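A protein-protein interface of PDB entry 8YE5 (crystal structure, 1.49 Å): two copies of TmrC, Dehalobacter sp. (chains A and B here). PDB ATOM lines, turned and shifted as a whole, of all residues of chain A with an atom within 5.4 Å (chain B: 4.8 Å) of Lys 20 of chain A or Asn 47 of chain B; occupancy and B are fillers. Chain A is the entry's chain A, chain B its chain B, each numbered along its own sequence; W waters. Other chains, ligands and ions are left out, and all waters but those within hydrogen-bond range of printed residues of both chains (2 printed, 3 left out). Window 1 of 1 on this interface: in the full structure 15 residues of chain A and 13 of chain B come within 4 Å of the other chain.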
ATOM      1  N   GLU A  13      19.954 -22.067   6.187  1.00  0.00           N
ATOM      2  CA  GLU A  13      20.838 -21.084   5.581  1.00  0.00           C
ATOM      3  C   GLU A  13      21.197 -21.479   4.159  1.00  0.00           C
ATOM      4  O   GLU A  13      21.406 -20.614   3.299  1.00  0.00           O
ATOM      5  CB  GLU A  13      22.088 -20.888   6.429  1.00  0.00           C
ATOM      6  CG  GLU A  13      21.861 -19.929   7.609  1.00  0.00           C
ATOM      7  CD  GLU A  13      21.872 -18.437   7.235  1.00  0.00           C
ATOM      8  OE1 GLU A  13      20.795 -17.797   7.227  1.00  0.00           O
ATOM      9  OE2 GLU A  13      22.941 -17.900   6.884  1.00  0.00           O
ATOM     10  N   GLY A  15      19.038 -22.919   2.202  1.00  0.00           N
ATOM     11  CA  GLY A  15      17.875 -22.418   1.492  1.00  0.00           C
ATOM     12  C   GLY A  15      17.974 -20.933   1.214  1.00  0.00           C
ATOM     13  O   GLY A  15      17.659 -20.481   0.116  1.00  0.00           O
ATOM     14  N   ASN A  16      18.446 -20.170   2.197  1.00  0.00           N
ATOM     15  CA  ASN A  16      18.608 -18.731   2.007  1.00  0.00           C
ATOM     16  C   ASN A  16      19.648 -18.431   0.931  1.00  0.00           C
ATOM     17  O   ASN A  16      19.450 -17.534   0.102  1.00  0.00           O
ATOM     18  CB  ASN A  16      19.022 -18.088   3.330  1.00  0.00           C
ATOM     19  CG  ASN A  16      17.906 -18.078   4.357  1.00  0.00           C
ATOM     20  OD1 ASN A  16      16.717 -18.210   4.030  1.00  0.00           O
ATOM     21  ND2 ASN A  16      18.284 -17.926   5.620  1.00  0.00           N
ATOM     22  N   GLU A  17      20.772 -19.157   0.933  1.00  0.00           N
ATOM     23  CA  GLU A  17      21.784 -18.938  -0.101  1.00  0.00           C
ATOM     24  C   GLU A  17      21.241 -19.271  -1.480  1.00  0.00           C
ATOM     25  O   GLU A  17      21.497 -18.552  -2.457  1.00  0.00           O
ATOM     26  CB  GLU A  17      23.028 -19.789   0.178  1.00  0.00           C
ATOM     27  CG  GLU A  17      23.852 -19.346   1.365  1.00  0.00           C
ATOM     28  CD  GLU A  17      24.343 -17.914   1.243  1.00  0.00           C
ATOM     29  OE1 GLU A  17      24.228 -17.157   2.231  1.00  0.00           O
ATOM     30  OE2 GLU A  17      24.831 -17.545   0.153  1.00  0.00           O
ATOM     31  N   ALA A  18      20.493 -20.368  -1.586  1.00  0.00           N
ATOM     32  CA  ALA A  18      19.903 -20.722  -2.865  1.00  0.00           C
ATOM     33  C   ALA A  18      18.911 -19.658  -3.304  1.00  0.00           C
ATOM     34  O   ALA A  18      18.850 -19.304  -4.487  1.00  0.00           O
ATOM     35  CB  ALA A  18      19.211 -22.081  -2.754  1.00  0.00           C
ATOM     36  N   PHE A  19      18.110 -19.153  -2.364  1.00  0.00           N
ATOM     37  CA  PHE A  19      17.142 -18.125  -2.720  1.00  0.00           C
ATOM     38  C   PHE A  19      17.845 -16.881  -3.257  1.00  0.00           C
ATOM     39  O   PHE A  19      17.391 -16.280  -4.235  1.00  0.00           O
ATOM     40  CB  PHE A  19      16.275 -17.781  -1.511  1.00  0.00           C
ATOM     41  CG  PHE A  19      15.186 -16.796  -1.819  1.00  0.00           C
ATOM     42  CD1 PHE A  19      15.433 -15.434  -1.770  1.00  0.00           C
ATOM     43  CD2 PHE A  19      13.918 -17.227  -2.154  1.00  0.00           C
ATOM     44  CE1 PHE A  19      14.439 -14.522  -2.070  1.00  0.00           C
ATOM     45  CE2 PHE A  19      12.917 -16.325  -2.439  1.00  0.00           C
ATOM     46  CZ  PHE A  19      13.172 -14.968  -2.403  1.00  0.00           C
ATOM     47  N   LYS A  20      18.964 -16.499  -2.634  1.00  0.00           N
ATOM     48  CA  LYS A  20      19.722 -15.322  -3.067  1.00  0.00           C
ATOM     49  C   LYS A  20      20.224 -15.471  -4.502  1.00  0.00           C
ATOM     50  O   LYS A  20      20.307 -14.483  -5.246  1.00  0.00           O
ATOM     51  CB  LYS A  20      20.904 -15.095  -2.123  1.00  0.00           C
ATOM     52  CG  LYS A  20      20.544 -14.542  -0.742  1.00  0.00           C
ATOM     53  CD  LYS A  20      21.761 -14.606   0.185  1.00  0.00           C
ATOM     54  CE  LYS A  20      21.391 -14.352   1.638  1.00  0.00           C
ATOM     55  NZ  LYS A  20      22.604 -14.383   2.509  1.00  0.00           N
ATOM     56  N   ALA A  21      20.570 -16.695  -4.909  1.00  0.00           N
ATOM     57  CA  ALA A  21      21.082 -16.978  -6.246  1.00  0.00           C
ATOM     58  C   ALA A  21      19.997 -17.136  -7.307  1.00  0.00           C
ATOM     59  O   ALA A  21      20.328 -17.326  -8.485  1.00  0.00           O
ATOM     60  CB  ALA A  21      21.923 -18.257  -6.215  1.00  0.00           C
ATOM     61  N   GLY A  22      18.717 -17.084  -6.943  1.00  0.00           N
ATOM     62  CA  GLY A  22      17.693 -17.400  -7.907  1.00  0.00           C
ATOM     63  C   GLY A  22      17.434 -18.876  -8.083  1.00  0.00           C
ATOM     64  O   GLY A  22      16.654 -19.250  -8.964  1.00  0.00           O
ATOM     65  N   ASN B  16      18.823 -11.551   9.242  1.00  0.00           N
ATOM     66  CA  ASN B  16      18.663 -11.757   7.804  1.00  0.00           C
ATOM     67  C   ASN B  16      17.586 -10.845   7.239  1.00  0.00           C
ATOM     68  O   ASN B  16      17.754 -10.274   6.157  1.00  0.00           O
ATOM     69  CB  ASN B  16      18.337 -13.218   7.494  1.00  0.00           C
ATOM     70  CG  ASN B  16      19.498 -14.158   7.772  1.00  0.00           C
ATOM     71  OD1 ASN B  16      20.653 -13.744   7.851  1.00  0.00           O
ATOM     72  ND2 ASN B  16      19.196 -15.445   7.901  1.00  0.00           N
ATOM     73  N   PHE B  19      19.064  -7.348   7.089  1.00  0.00           N
ATOM     74  CA  PHE B  19      19.958  -7.215   5.949  1.00  0.00           C
ATOM     75  C   PHE B  19      19.165  -7.067   4.651  1.00  0.00           C
ATOM     76  O   PHE B  19      19.486  -6.214   3.818  1.00  0.00           O
ATOM     77  CB  PHE B  19      20.894  -8.419   5.877  1.00  0.00           C
ATOM     78  CG  PHE B  19      21.942  -8.287   4.819  1.00  0.00           C
ATOM     79  CD1 PHE B  19      21.675  -8.615   3.499  1.00  0.00           C
ATOM     80  CD2 PHE B  19      23.208  -7.843   5.148  1.00  0.00           C
ATOM     81  CE1 PHE B  19      22.644  -8.470   2.524  1.00  0.00           C
ATOM     82  CE2 PHE B  19      24.181  -7.701   4.183  1.00  0.00           C
ATOM     83  CZ  PHE B  19      23.901  -8.020   2.864  1.00  0.00           C
ATOM     84  N   TYR B  31      23.115 -10.048  14.297  1.00  0.00           N
ATOM     85  CA  TYR B  31      24.099 -11.086  14.011  1.00  0.00           C
ATOM     86  C   TYR B  31      25.102 -11.201  15.149  1.00  0.00           C
ATOM     87  O   TYR B  31      25.524 -12.307  15.495  1.00  0.00           O
ATOM     88  CB  TYR B  31      24.840 -10.750  12.718  1.00  0.00           C
ATOM     89  CG  TYR B  31      24.062 -10.939  11.437  1.00  0.00           C
ATOM     90  CD1 TYR B  31      23.083 -11.925  11.317  1.00  0.00           C
ATOM     91  CD2 TYR B  31      24.331 -10.138  10.342  1.00  0.00           C
ATOM     92  CE1 TYR B  31      22.399 -12.107  10.112  1.00  0.00           C
ATOM     93  CE2 TYR B  31      23.649 -10.302   9.137  1.00  0.00           C
ATOM     94  CZ  TYR B  31      22.688 -11.280   9.035  1.00  0.00           C
ATOM     95  OH  TYR B  31      22.038 -11.440   7.826  1.00  0.00           O
ATOM     96  N   PHE B  43      27.926 -19.102   8.056  1.00  0.00           N
ATOM     97  CA  PHE B  43      26.919 -18.236   7.457  1.00  0.00           C
ATOM     98  C   PHE B  43      26.760 -16.945   8.243  1.00  0.00           C
ATOM     99  O   PHE B  43      26.663 -15.870   7.648  1.00  0.00           O
ATOM    100  CB  PHE B  43      25.583 -18.979   7.385  1.00  0.00           C
ATOM    101  CG  PHE B  43      25.631 -20.214   6.567  1.00  0.00           C
ATOM    102  CD1 PHE B  43      25.563 -20.150   5.188  1.00  0.00           C
ATOM    103  CD2 PHE B  43      25.764 -21.445   7.175  1.00  0.00           C
ATOM    104  CE1 PHE B  43      25.613 -21.303   4.423  1.00  0.00           C
ATOM    105  CE2 PHE B  43      25.818 -22.597   6.412  1.00  0.00           C
ATOM    106  CZ  PHE B  43      25.748 -22.522   5.042  1.00  0.00           C
ATOM    107  N   LEU B  44      26.705 -17.029   9.577  1.00  0.00           N
ATOM    108  CA  LEU B  44      26.543 -15.821  10.375  1.00  0.00           C
ATOM    109  C   LEU B  44      27.733 -14.902  10.181  1.00  0.00           C
ATOM    110  O   LEU B  44      27.575 -13.682  10.063  1.00  0.00           O
ATOM    111  CB  LEU B  44      26.407 -16.174  11.863  1.00  0.00           C
ATOM    112  CG  LEU B  44      25.018 -16.544  12.387  1.00  0.00           C
ATOM    113  CD1 LEU B  44      25.115 -16.947  13.843  1.00  0.00           C
ATOM    114  CD2 LEU B  44      24.046 -15.390  12.191  1.00  0.00           C
ATOM    115  N   TYR B  45      28.937 -15.465  10.200  1.00  0.00           N
ATOM    116  CA  TYR B  45      30.114 -14.622  10.065  1.00  0.00           C
ATOM    117  C   TYR B  45      30.195 -14.015   8.673  1.00  0.00           C
ATOM    118  O   TYR B  45      30.617 -12.864   8.520  1.00  0.00           O
ATOM    119  CB  TYR B  45      31.354 -15.449  10.359  1.00  0.00           C
ATOM    120  CG  TYR B  45      31.694 -15.531  11.812  1.00  0.00           C
ATOM    121  CD1 TYR B  45      31.990 -14.393  12.542  1.00  0.00           C
ATOM    122  CD2 TYR B  45      31.712 -16.753  12.458  1.00  0.00           C
ATOM    123  CE1 TYR B  45      32.313 -14.471  13.882  1.00  0.00           C
ATOM    124  CE2 TYR B  45      32.031 -16.841  13.802  1.00  0.00           C
ATOM    125  CZ  TYR B  45      32.335 -15.695  14.499  1.00  0.00           C
ATOM    126  OH  TYR B  45      32.663 -15.749  15.840  1.00  0.00           O
ATOM    127  N   THR B  46      29.814 -14.779   7.647  1.00  0.00           N
ATOM    128  CA  THR B  46      29.840 -14.221   6.301  1.00  0.00           C
ATOM    129  C   THR B  46      28.787 -13.135   6.136  1.00  0.00           C
ATOM    130  O   THR B  46      29.052 -12.100   5.517  1.00  0.00           O
ATOM    131  CB  THR B  46      29.662 -15.328   5.277  1.00  0.00           C
ATOM    132  OG1 THR B  46      30.770 -16.232   5.390  1.00  0.00           O
ATOM    133  CG2 THR B  46      29.610 -14.758   3.883  1.00  0.00           C
ATOM    134  N   ASN B  47      27.603 -13.335   6.716  1.00  0.00           N
ATOM    135  CA  ASN B  47      26.554 -12.326   6.606  1.00  0.00           C
ATOM    136  C   ASN B  47      26.921 -11.071   7.379  1.00  0.00           C
ATOM    137  O   ASN B  47      26.719  -9.961   6.884  1.00  0.00           O
ATOM    138  CB  ASN B  47      25.228 -12.912   7.093  1.00  0.00           C
ATOM    139  CG  ASN B  47      24.643 -13.880   6.100  1.00  0.00           C
ATOM    140  OD1 ASN B  47      25.027 -13.874   4.935  1.00  0.00           O
ATOM    141  ND2 ASN B  47      23.748 -14.737   6.557  1.00  0.00           N
ATOM    142  N   ARG B  48      27.505 -11.221   8.572  1.00  0.00           N
ATOM    143  CA  ARG B  48      27.948 -10.022   9.271  1.00  0.00           C
ATOM    144  C   ARG B  48      29.113  -9.360   8.545  1.00  0.00           C
ATOM    145  O   ARG B  48      29.196  -8.127   8.527  1.00  0.00           O
ATOM    146  CB  ARG B  48      28.272 -10.310  10.738  1.00  0.00           C
ATOM    147  CG  ARG B  48      28.367  -9.019  11.557  1.00  0.00           C
ATOM    148  CD  ARG B  48      28.584  -9.288  13.038  1.00  0.00           C
ATOM    149  NE  ARG B  48      29.909  -9.835  13.299  1.00  0.00           N
ATOM    150  CZ  ARG B  48      30.374 -10.098  14.509  1.00  0.00           C
ATOM    151  NH1 ARG B  48      29.666  -9.814  15.593  1.00  0.00           N
ATOM    152  NH2 ARG B  48      31.577 -10.648  14.639  1.00  0.00           N
ATOM    153  N   SER B  49      30.004 -10.147   7.935  1.00  0.00           N
ATOM    154  CA  SER B  49      31.071  -9.570   7.122  1.00  0.00           C
ATOM    155  C   SER B  49      30.490  -8.703   6.015  1.00  0.00           C
ATOM    156  O   SER B  49      30.991  -7.605   5.733  1.00  0.00           O
ATOM    157  CB  SER B  49      31.920 -10.683   6.494  1.00  0.00           C
ATOM    158  OG  SER B  49      32.812 -10.131   5.545  1.00  0.00           O
ATOM    159  N   PHE B  50      29.428  -9.182   5.373  1.00  0.00           N
ATOM    160  CA  PHE B  50      28.814  -8.441   4.284  1.00  0.00           C
ATOM    161  C   PHE B  50      28.200  -7.148   4.801  1.00  0.00           C
ATOM    162  O   PHE B  50      28.387  -6.080   4.207  1.00  0.00           O
ATOM    163  CB  PHE B  50      27.781  -9.375   3.639  1.00  0.00           C
ATOM    164  CG  PHE B  50      27.347  -9.002   2.241  1.00  0.00           C
ATOM    165  CD1 PHE B  50      26.647  -9.917   1.483  1.00  0.00           C
ATOM    166  CD2 PHE B  50      27.635  -7.774   1.685  1.00  0.00           C
ATOM    167  CE1 PHE B  50      26.229  -9.610   0.203  1.00  0.00           C
ATOM    168  CE2 PHE B  50      27.215  -7.467   0.392  1.00  0.00           C
ATOM    169  CZ  PHE B  50      26.515  -8.388  -0.339  1.00  0.00           C
ATOM    170  N   ALA B  51      27.497  -7.215   5.930  1.00  0.00           N
ATOM    171  CA  ALA B  51      26.920  -6.003   6.514  1.00  0.00           C
ATOM    172  C   ALA B  51      27.999  -4.981   6.856  1.00  0.00           C
ATOM    173  O   ALA B  51      27.850  -3.783   6.580  1.00  0.00           O
ATOM    174  CB  ALA B  51      26.097  -6.379   7.745  1.00  0.00           C
ATOM    175  N   LYS B  77      31.804 -18.260  -0.201  1.00  0.00           N
ATOM    176  CA  LYS B  77      31.397 -16.895   0.104  1.00  0.00           C
ATOM    177  C   LYS B  77      32.273 -16.278   1.178  1.00  0.00           C
ATOM    178  O   LYS B  77      32.501 -15.062   1.170  1.00  0.00           O
ATOM    179  CB  LYS B  77      29.933 -16.877   0.527  1.00  0.00           C
ATOM    180  CG  LYS B  77      29.292 -15.518   0.368  1.00  0.00           C
ATOM    181  CD  LYS B  77      27.818 -15.598   0.751  1.00  0.00           C
ATOM    182  CE  LYS B  77      27.243 -14.234   1.107  1.00  0.00           C
ATOM    183  NZ  LYS B  77      25.801 -14.127   0.750  1.00  0.00           N
HETATM  184  O   HOH W   1      21.006 -15.142   4.955  1.00  0.00           O
HETATM  185  O   HOH W   2      22.913 -15.505   8.695  1.00  0.00           O
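Water W2 lies within hydrogen-bond range of the side-chain amide nitrogen (ND2) of Asn 47 of chain B (2.4 Å), the side-chain amide oxygen (OD1) of Asn 16 of chain B (3.0 Å) and the side-chain carboxylate (OE2) of Glu 13 of chain A (3.0 Å). Water W1 lies within hydrogen-bond range of the side-chain amino group (NZ) of Lys 20 of chain A (3.0 Å), the side-chain amide nitrogen (ND2) of Asn 47 of chain B (3.2 Å) and the side-chain amide oxygen (OD1) of Asn 16 of chain B (3.2 Å).
The side-chain carboxylate of Glu 13 of chain A lies within hydrogen-bond range of the side-chain amide nitrogen of Asn 16 of chain B, 2.9 Å away. The side-chain carboxylate (OE2) of Glu 13 of chain A is in hydrogen-bond range of the side-chain amide nitrogen (ND2) of Asn 47 of chain B. ND2 of Asn 16 of chain A sits close to ND2 of Asn 16 of chain B (3.5 Å). OE2 of Glu 17 of chain A lies within salt-bridge range of NZ of Lys 77 of chain B, at 3.6 Å. The side-chain amide oxygen (OD1) of Asn 47 of chain B is in hydrogen-bond range of the side-chain amino group (NZ) of Lys 20 of chain A, 3.5 Å away.
Asn 16 of chain B touches its own counterpart, Asn 16 of chain A. Positions printed for both chains: 16 and 19. Of the 7 pairs that touch across the chains among the printed residues, 1 has its exchanged pair printed and touching as well.
The side-chain amide nitrogen (ND2) of Asn 16 of chain A sits at hydrogen-bond distance from the side-chain carboxylate (OE1) of Glu 13 of chain A. The side-chain carboxylate (OE1) of Glu 17 of chain A lies within salt-bridge range of the side-chain amino group (NZ) of Lys 20 of chain A, 3.2 Å away. The side-chain amide oxygen of Asn 16 of chain B is in hydrogen-bond range of the side-chain hydroxyl of Tyr 31 of chain B. OD1 of Asn 16 of chain B sits at hydrogen-bond distance from ND2 of Asn 47 of chain B (3.5 Å). The side-chain amide nitrogen (ND2) of Asn 47 of chain B sits close to the backbone carbonyl oxygen (O) of Phe 43 of chain B.
Printed residues of chain B within 4 Å of Asn 16 of chain A: Asn 16. Printed residues of chain B within 4 Å of Glu 17 of chain A: Lys 77. Of chain B, only Asn 47 (3.5 Å) and Lys 77 (3.7 Å) come within 4 Å of Lys 20 of chain A. Printed residues of chain A within 4 Å of Asn 47 of chain B: Glu 13 (3.3 Å) and Lys 20 (3.5 Å). The nearest printed residue of chain B that does not touch Lys 20 of chain A is Asn 16 of chain B (5.7 Å). The nearest printed residue of chain B that does not touch Glu 17 of chain A is Phe 43 of chain B (4.04 Å).
Of the 13 printed residues of chain B, 4 touch a printed residue of chain A. Printed residues of chain B that touch a printed residue of chain A: Asn 16, Phe 43, Asn 47 and Lys 77. Printed residues of chain A that touch a printed residue of chain B: Glu 13, Asn 16, Glu 17 and Lys 20.
Among the printed residues, pairs that only touch across the chains: Glu 13 of chain A with Phe 43 of chain B (2.9 Å) and Lys 20 of chain A with Lys 77 of chain B (3.7 Å).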
